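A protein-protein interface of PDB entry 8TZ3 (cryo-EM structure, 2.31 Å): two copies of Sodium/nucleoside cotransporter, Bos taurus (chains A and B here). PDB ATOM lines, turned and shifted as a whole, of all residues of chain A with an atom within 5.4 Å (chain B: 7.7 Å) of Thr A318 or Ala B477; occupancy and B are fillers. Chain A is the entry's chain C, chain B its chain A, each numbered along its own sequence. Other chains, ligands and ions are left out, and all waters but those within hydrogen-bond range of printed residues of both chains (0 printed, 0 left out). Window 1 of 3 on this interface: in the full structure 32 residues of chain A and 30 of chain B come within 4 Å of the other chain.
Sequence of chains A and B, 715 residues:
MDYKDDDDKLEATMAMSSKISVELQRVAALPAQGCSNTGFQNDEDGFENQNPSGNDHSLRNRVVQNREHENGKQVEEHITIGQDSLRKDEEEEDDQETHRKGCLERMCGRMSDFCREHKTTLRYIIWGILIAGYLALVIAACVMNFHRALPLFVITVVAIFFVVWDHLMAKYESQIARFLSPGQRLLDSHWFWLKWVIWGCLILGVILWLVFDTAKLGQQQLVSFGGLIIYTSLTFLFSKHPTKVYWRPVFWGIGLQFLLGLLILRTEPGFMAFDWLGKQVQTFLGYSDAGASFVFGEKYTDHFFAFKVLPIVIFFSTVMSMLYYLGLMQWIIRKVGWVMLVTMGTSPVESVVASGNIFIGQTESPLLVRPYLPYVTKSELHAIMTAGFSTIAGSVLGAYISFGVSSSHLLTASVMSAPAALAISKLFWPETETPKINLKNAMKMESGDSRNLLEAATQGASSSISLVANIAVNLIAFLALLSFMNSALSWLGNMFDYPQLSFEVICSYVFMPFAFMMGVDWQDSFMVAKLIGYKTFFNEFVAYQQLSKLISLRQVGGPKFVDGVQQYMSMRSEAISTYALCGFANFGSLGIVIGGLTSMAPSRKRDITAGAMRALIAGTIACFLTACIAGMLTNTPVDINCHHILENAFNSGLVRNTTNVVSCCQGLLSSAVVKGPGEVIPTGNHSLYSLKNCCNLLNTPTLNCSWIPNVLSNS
No position is printed for both chains.
Of the 7 pairs that touch across the chains among the printed residues, none has its exchanged pair printed and touching as well.
The side-chain hydroxyl (OG) of Ser B483 lies within hydrogen-bond range of the backbone carbonyl oxygen (O) of Ala B480 (2.5 Å).
The side-chain hydroxyl (OG1) of Thr A318 lies within hydrogen-bond range of the backbone carbonyl oxygen (O) of Ile A314 (2.9 Å).
The side-chain hydroxyl (OG) of Ser A321 is in hydrogen-bond range of the backbone carbonyl oxygen (O) of Thr A318 (2.7 Å).
Hydrophobic or aromatic side chains of chain A that line the printed part of chain B: Ile A314, Phe A315, Met A322 and Ala A461.
Of the 14 printed residues of chain B, 5 touch a printed residue of chain A.
Hydrophobic or aromatic side chains of chain B within 4 Å of the printed part of chain A: Val B473, Ala B477, Ala B480 and Leu B481.
Among the printed residues, 7 pairs touch across the chains.
Printed residues of chain B within 4 Å of Ile A314: Val B473.
Of chain B, only Ala B477 comes within 4 Å of Thr A318.
Of the printed residues of chain A, Asn B474 touches Ala A461.
Ala B477 touches just one residue of chain A: Thr A318 (3.6 Å).
Of the printed residues of chain A, Ala B480 touches Phe A315 (3.6 Å).
The nearest residue of chain B that does not touch Thr A318 is Leu B481 (4.3 Å).
The nearest residue of chain A that does not touch Ala B477 is Ala A461 (4.2 Å).
The nearest printed residue of chain A that does not touch Ala B480 is Ile A314 (7.4 Å).
Among the printed residues, pairs that only touch across the chains: Ala A461 with Val B473, Ile A314 with Val B473, Thr A318 with Ala B477, Ala A461 with Asn B474, Phe A315 with Ala B480, Phe A315 with Leu B481 and Met A322 with Leu B481.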
ATOM      1  N   VAL A 313      16.017   8.442  11.196  1.00  0.00           N
ATOM      2  CA  VAL A 313      15.367   8.102  12.457  1.00  0.00           C
ATOM      3  C   VAL A 313      16.372   7.488  13.425  1.00  0.00           C
ATOM      4  O   VAL A 313      16.301   7.707  14.638  1.00  0.00           O
ATOM      5  CB  VAL A 313      14.167   7.170  12.191  1.00  0.00           C
ATOM      6  CG1 VAL A 313      13.423   6.842  13.456  1.00  0.00           C
ATOM      7  CG2 VAL A 313      13.227   7.785  11.189  1.00  0.00           C
ATOM      8  N   ILE A 314      17.320   6.714  12.903  1.00  0.00           N
ATOM      9  CA  ILE A 314      18.386   6.148  13.723  1.00  0.00           C
ATOM     10  C   ILE A 314      19.285   7.250  14.272  1.00  0.00           C
ATOM     11  O   ILE A 314      19.625   7.263  15.460  1.00  0.00           O
ATOM     12  CB  ILE A 314      19.179   5.112  12.903  1.00  0.00           C
ATOM     13  CG1 ILE A 314      18.267   3.946  12.523  1.00  0.00           C
ATOM     14  CG2 ILE A 314      20.423   4.634  13.640  1.00  0.00           C
ATOM     15  CD1 ILE A 314      18.763   3.103  11.418  1.00  0.00           C
ATOM     16  N   PHE A 315      19.688   8.186  13.414  1.00  0.00           N
ATOM     17  CA  PHE A 315      20.597   9.247  13.830  1.00  0.00           C
ATOM     18  C   PHE A 315      19.949  10.182  14.846  1.00  0.00           C
ATOM     19  O   PHE A 315      20.567  10.539  15.853  1.00  0.00           O
ATOM     20  CB  PHE A 315      21.080  10.016  12.600  1.00  0.00           C
ATOM     21  CG  PHE A 315      22.061  11.106  12.902  1.00  0.00           C
ATOM     22  CD1 PHE A 315      23.130  10.894  13.751  1.00  0.00           C
ATOM     23  CD2 PHE A 315      21.924  12.342  12.318  1.00  0.00           C
ATOM     24  CE1 PHE A 315      24.014  11.895  14.015  1.00  0.00           C
ATOM     25  CE2 PHE A 315      22.814  13.342  12.583  1.00  0.00           C
ATOM     26  CZ  PHE A 315      23.860  13.120  13.430  1.00  0.00           C
ATOM     27  N   PHE A 316      18.708  10.600  14.598  1.00  0.00           N
ATOM     28  CA  PHE A 316      18.033  11.496  15.531  1.00  0.00           C
ATOM     29  C   PHE A 316      17.787  10.819  16.871  1.00  0.00           C
ATOM     30  O   PHE A 316      17.922  11.451  17.922  1.00  0.00           O
ATOM     31  CB  PHE A 316      16.719  11.991  14.931  1.00  0.00           C
ATOM     32  CG  PHE A 316      16.871  13.152  13.993  1.00  0.00           C
ATOM     33  CD1 PHE A 316      18.008  13.321  13.239  1.00  0.00           C
ATOM     34  CD2 PHE A 316      15.870  14.082  13.876  1.00  0.00           C
ATOM     35  CE1 PHE A 316      18.131  14.386  12.389  1.00  0.00           C
ATOM     36  CE2 PHE A 316      15.992  15.147  13.029  1.00  0.00           C
ATOM     37  CZ  PHE A 316      17.122  15.299  12.282  1.00  0.00           C
ATOM     38  N   SER A 317      17.419   9.539  16.856  1.00  0.00           N
ATOM     39  CA  SER A 317      17.278   8.790  18.098  1.00  0.00           C
ATOM     40  C   SER A 317      18.596   8.716  18.861  1.00  0.00           C
ATOM     41  O   SER A 317      18.620   8.845  20.088  1.00  0.00           O
ATOM     42  CB  SER A 317      16.748   7.391  17.795  1.00  0.00           C
ATOM     43  OG  SER A 317      15.657   7.440  16.905  1.00  0.00           O
ATOM     44  N   THR A 318      19.698   8.486  18.150  1.00  0.00           N
ATOM     45  CA  THR A 318      21.020   8.509  18.764  1.00  0.00           C
ATOM     46  C   THR A 318      21.311   9.852  19.426  1.00  0.00           C
ATOM     47  O   THR A 318      21.813   9.900  20.552  1.00  0.00           O
ATOM     48  CB  THR A 318      22.073   8.177  17.701  1.00  0.00           C
ATOM     49  OG1 THR A 318      21.852   6.858  17.203  1.00  0.00           O
ATOM     50  CG2 THR A 318      23.468   8.271  18.236  1.00  0.00           C
ATOM     51  N   VAL A 319      21.005  10.952  18.741  1.00  0.00           N
ATOM     52  CA  VAL A 319      21.316  12.279  19.259  1.00  0.00           C
ATOM     53  C   VAL A 319      20.466  12.607  20.481  1.00  0.00           C
ATOM     54  O   VAL A 319      20.952  13.211  21.442  1.00  0.00           O
ATOM     55  CB  VAL A 319      21.138  13.325  18.147  1.00  0.00           C
ATOM     56  CG1 VAL A 319      21.211  14.724  18.698  1.00  0.00           C
ATOM     57  CG2 VAL A 319      22.165  13.120  17.077  1.00  0.00           C
ATOM     58  N   MET A 320      19.186  12.239  20.458  1.00  0.00           N
ATOM     59  CA  MET A 320      18.314  12.516  21.591  1.00  0.00           C
ATOM     60  C   MET A 320      18.786  11.799  22.850  1.00  0.00           C
ATOM     61  O   MET A 320      18.652  12.329  23.957  1.00  0.00           O
ATOM     62  CB  MET A 320      16.879  12.120  21.252  1.00  0.00           C
ATOM     63  CG  MET A 320      16.243  12.927  20.136  1.00  0.00           C
ATOM     64  SD  MET A 320      16.178  14.697  20.435  1.00  0.00           S
ATOM     65  CE  MET A 320      15.016  14.735  21.783  1.00  0.00           C
ATOM     66  N   SER A 321      19.334  10.592  22.706  1.00  0.00           N
ATOM     67  CA  SER A 321      19.836   9.863  23.864  1.00  0.00           C
ATOM     68  C   SER A 321      21.094  10.511  24.431  1.00  0.00           C
ATOM     69  O   SER A 321      21.353  10.427  25.635  1.00  0.00           O
ATOM     70  CB  SER A 321      20.100   8.407  23.486  1.00  0.00           C
ATOM     71  OG  SER A 321      21.258   8.283  22.695  1.00  0.00           O
ATOM     72  N   MET A 322      21.889  11.156  23.578  1.00  0.00           N
ATOM     73  CA  MET A 322      23.069  11.869  24.049  1.00  0.00           C
ATOM     74  C   MET A 322      22.691  13.128  24.819  1.00  0.00           C
ATOM     75  O   MET A 322      23.359  13.491  25.791  1.00  0.00           O
ATOM     76  CB  MET A 322      23.971  12.219  22.868  1.00  0.00           C
ATOM     77  CG  MET A 322      24.417  11.025  22.054  1.00  0.00           C
ATOM     78  SD  MET A 322      25.145  11.435  20.466  1.00  0.00           S
ATOM     79  CE  MET A 322      26.793  11.852  20.991  1.00  0.00           C
ATOM     80  N   ALA A 456      25.812   6.229  25.615  1.00  0.00           N
ATOM     81  CA  ALA A 456      24.499   6.807  25.356  1.00  0.00           C
ATOM     82  C   ALA A 456      24.190   6.830  23.866  1.00  0.00           C
ATOM     83  O   ALA A 456      23.022   6.787  23.467  1.00  0.00           O
ATOM     84  CB  ALA A 456      24.422   8.212  25.946  1.00  0.00           C
ATOM     85  N   ALA A 457      25.226   6.905  23.031  1.00  0.00           N
ATOM     86  CA  ALA A 457      25.033   6.853  21.590  1.00  0.00           C
ATOM     87  C   ALA A 457      24.624   5.459  21.125  1.00  0.00           C
ATOM     88  O   ALA A 457      23.778   5.318  20.238  1.00  0.00           O
ATOM     89  CB  ALA A 457      26.309   7.304  20.888  1.00  0.00           C
ATOM     90  N   GLY A 460      20.955   4.532  22.118  1.00  0.00           N
ATOM     91  CA  GLY A 460      19.951   5.175  21.292  1.00  0.00           C
ATOM     92  C   GLY A 460      19.857   4.570  19.908  1.00  0.00           C
ATOM     93  O   GLY A 460      18.786   4.552  19.299  1.00  0.00           O
ATOM     94  N   ALA A 461      20.981   4.087  19.386  1.00  0.00           N
ATOM     95  CA  ALA A 461      20.971   3.363  18.125  1.00  0.00           C
ATOM     96  C   ALA A 461      20.291   2.006  18.273  1.00  0.00           C
ATOM     97  O   ALA A 461      19.468   1.618  17.439  1.00  0.00           O
ATOM     98  CB  ALA A 461      22.401   3.218  17.611  1.00  0.00           C
ATOM     99  N   ILE B 471      25.332  -4.235  14.451  1.00  0.00           N
ATOM    100  CA  ILE B 471      26.485  -3.810  13.663  1.00  0.00           C
ATOM    101  C   ILE B 471      26.083  -2.706  12.691  1.00  0.00           C
ATOM    102  O   ILE B 471      26.755  -1.676  12.583  1.00  0.00           O
ATOM    103  CB  ILE B 471      27.117  -5.012  12.929  1.00  0.00           C
ATOM    104  CG1 ILE B 471      27.768  -5.984  13.910  1.00  0.00           C
ATOM    105  CG2 ILE B 471      28.154  -4.561  11.927  1.00  0.00           C
ATOM    106  CD1 ILE B 471      28.049  -7.356  13.335  1.00  0.00           C
ATOM    107  N   ALA B 472      24.977  -2.905  11.974  1.00  0.00           N
ATOM    108  CA  ALA B 472      24.572  -1.966  10.935  1.00  0.00           C
ATOM    109  C   ALA B 472      24.141  -0.624  11.514  1.00  0.00           C
ATOM    110  O   ALA B 472      24.449   0.428  10.945  1.00  0.00           O
ATOM    111  CB  ALA B 472      23.449  -2.575  10.104  1.00  0.00           C
ATOM    112  N   VAL B 473      23.421  -0.637  12.633  1.00  0.00           N
ATOM    113  CA  VAL B 473      22.862   0.597  13.174  1.00  0.00           C
ATOM    114  C   VAL B 473      23.932   1.415  13.887  1.00  0.00           C
ATOM    115  O   VAL B 473      23.917   2.649  13.837  1.00  0.00           O
ATOM    116  CB  VAL B 473      21.663   0.267  14.087  1.00  0.00           C
ATOM    117  CG1 VAL B 473      21.123   1.461  14.730  1.00  0.00           C
ATOM    118  CG2 VAL B 473      20.554  -0.338  13.280  1.00  0.00           C
ATOM    119  N   ASN B 474      24.866   0.755  14.569  1.00  0.00           N
ATOM    120  CA  ASN B 474      25.962   1.475  15.205  1.00  0.00           C
ATOM    121  C   ASN B 474      26.864   2.151  14.180  1.00  0.00           C
ATOM    122  O   ASN B 474      27.457   3.196  14.462  1.00  0.00           O
ATOM    123  CB  ASN B 474      26.766   0.525  16.083  1.00  0.00           C
ATOM    124  CG  ASN B 474      26.120   0.285  17.414  1.00  0.00           C
ATOM    125  OD1 ASN B 474      25.031   0.773  17.698  1.00  0.00           O
ATOM    126  ND2 ASN B 474      26.790  -0.483  18.242  1.00  0.00           N
ATOM    127  N   LEU B 475      26.983   1.572  12.988  1.00  0.00           N
ATOM    128  CA  LEU B 475      27.812   2.171  11.950  1.00  0.00           C
ATOM    129  C   LEU B 475      27.110   3.340  11.270  1.00  0.00           C
ATOM    130  O   LEU B 475      27.759   4.320  10.894  1.00  0.00           O
ATOM    131  CB  LEU B 475      28.209   1.108  10.929  1.00  0.00           C
ATOM    132  CG  LEU B 475      29.402   0.209  11.231  1.00  0.00           C
ATOM    133  CD1 LEU B 475      29.370  -0.955  10.284  1.00  0.00           C
ATOM    134  CD2 LEU B 475      30.707   0.946  11.113  1.00  0.00           C
ATOM    135  N   ILE B 476      25.791   3.256  11.087  1.00  0.00           N
ATOM    136  CA  ILE B 476      25.041   4.409  10.600  1.00  0.00           C
ATOM    137  C   ILE B 476      25.172   5.570  11.575  1.00  0.00           C
ATOM    138  O   ILE B 476      25.390   6.718  11.171  1.00  0.00           O
ATOM    139  CB  ILE B 476      23.566   4.030  10.355  1.00  0.00           C
ATOM    140  CG1 ILE B 476      23.448   3.073   9.168  1.00  0.00           C
ATOM    141  CG2 ILE B 476      22.705   5.263  10.113  1.00  0.00           C
ATOM    142  CD1 ILE B 476      22.197   2.258   9.150  1.00  0.00           C
ATOM    143  N   ALA B 477      25.057   5.290  12.870  1.00  0.00           N
ATOM    144  CA  ALA B 477      25.115   6.338  13.880  1.00  0.00           C
ATOM    145  C   ALA B 477      26.525   6.903  14.033  1.00  0.00           C
ATOM    146  O   ALA B 477      26.713   8.123  14.026  1.00  0.00           O
ATOM    147  CB  ALA B 477      24.598   5.796  15.205  1.00  0.00           C
ATOM    148  N   PHE B 478      27.528   6.036  14.183  1.00  0.00           N
ATOM    149  CA  PHE B 478      28.892   6.511  14.399  1.00  0.00           C
ATOM    150  C   PHE B 478      29.400   7.327  13.220  1.00  0.00           C
ATOM    151  O   PHE B 478      30.106   8.322  13.408  1.00  0.00           O
ATOM    152  CB  PHE B 478      29.832   5.332  14.667  1.00  0.00           C
ATOM    153  CG  PHE B 478      29.794   4.805  16.072  1.00  0.00           C
ATOM    154  CD1 PHE B 478      29.418   5.597  17.137  1.00  0.00           C
ATOM    155  CD2 PHE B 478      30.159   3.499  16.327  1.00  0.00           C
ATOM    156  CE1 PHE B 478      29.398   5.094  18.409  1.00  0.00           C
ATOM    157  CE2 PHE B 478      30.134   3.000  17.593  1.00  0.00           C
ATOM    158  CZ  PHE B 478      29.756   3.794  18.635  1.00  0.00           C
ATOM    159  N   LEU B 479      29.065   6.923  11.997  1.00  0.00           N
ATOM    160  CA  LEU B 479      29.594   7.611  10.829  1.00  0.00           C
ATOM    161  C   LEU B 479      28.833   8.894  10.531  1.00  0.00           C
ATOM    162  O   LEU B 479      29.368   9.785   9.868  1.00  0.00           O
ATOM    163  CB  LEU B 479      29.575   6.673   9.627  1.00  0.00           C
ATOM    164  CG  LEU B 479      30.544   5.489   9.660  1.00  0.00           C
ATOM    165  CD1 LEU B 479      30.277   4.580   8.501  1.00  0.00           C
ATOM    166  CD2 LEU B 479      31.981   5.932   9.645  1.00  0.00           C
ATOM    167  N   ALA B 480      27.593   9.003  11.005  1.00  0.00           N
ATOM    168  CA  ALA B 480      26.871  10.262  10.917  1.00  0.00           C
ATOM    169  C   ALA B 480      27.361  11.263  11.960  1.00  0.00           C
ATOM    170  O   ALA B 480      27.441  12.464  11.682  1.00  0.00           O
ATOM    171  CB  ALA B 480      25.379  10.004  11.067  1.00  0.00           C
ATOM    172  N   LEU B 481      27.681  10.789  13.166  1.00  0.00           N
ATOM    173  CA  LEU B 481      28.279  11.647  14.184  1.00  0.00           C
ATOM    174  C   LEU B 481      29.629  12.194  13.742  1.00  0.00           C
ATOM    175  O   LEU B 481      29.940  13.365  13.982  1.00  0.00           O
ATOM    176  CB  LEU B 481      28.435  10.875  15.489  1.00  0.00           C
ATOM    177  CG  LEU B 481      27.188  10.584  16.307  1.00  0.00           C
ATOM    178  CD1 LEU B 481      27.509   9.613  17.419  1.00  0.00           C
ATOM    179  CD2 LEU B 481      26.608  11.864  16.861  1.00  0.00           C
ATOM    180  N   LEU B 482      30.460  11.352  13.129  1.00  0.00           N
ATOM    181  CA  LEU B 482      31.755  11.799  12.637  1.00  0.00           C
ATOM    182  C   LEU B 482      31.610  12.904  11.601  1.00  0.00           C
ATOM    183  O   LEU B 482      32.343  13.896  11.639  1.00  0.00           O
ATOM    184  CB  LEU B 482      32.511  10.608  12.063  1.00  0.00           C
ATOM    185  CG  LEU B 482      33.926  10.801  11.529  1.00  0.00           C
ATOM    186  CD1 LEU B 482      34.876  11.228  12.612  1.00  0.00           C
ATOM    187  CD2 LEU B 482      34.379   9.534  10.897  1.00  0.00           C
ATOM    188  N   SER B 483      30.678  12.748  10.659  1.00  0.00           N
ATOM    189  CA  SER B 483      30.443  13.787   9.666  1.00  0.00           C
ATOM    190  C   SER B 483      30.037  15.101  10.322  1.00  0.00           C
ATOM    191  O   SER B 483      30.450  16.177   9.880  1.00  0.00           O
ATOM    192  CB  SER B 483      29.377  13.324   8.676  1.00  0.00           C
ATOM    193  OG  SER B 483      28.256  12.807   9.354  1.00  0.00           O
ATOM    194  N   PHE B 538      35.024   5.014  18.559  1.00  0.00           N
ATOM    195  CA  PHE B 538      33.954   4.328  17.840  1.00  0.00           C
ATOM    196  C   PHE B 538      34.071   2.820  18.000  1.00  0.00           C
ATOM    197  O   PHE B 538      33.843   2.310  19.097  1.00  0.00           O
ATOM    198  CB  PHE B 538      33.961   4.740  16.371  1.00  0.00           C
ATOM    199  CG  PHE B 538      33.799   6.203  16.164  1.00  0.00           C
ATOM    200  CD1 PHE B 538      32.655   6.849  16.572  1.00  0.00           C
ATOM    201  CD2 PHE B 538      34.796   6.938  15.574  1.00  0.00           C
ATOM    202  CE1 PHE B 538      32.511   8.189  16.390  1.00  0.00           C
ATOM    203  CE2 PHE B 538      34.655   8.280  15.391  1.00  0.00           C
ATOM    204  CZ  PHE B 538      33.510   8.907  15.798  1.00  0.00           C
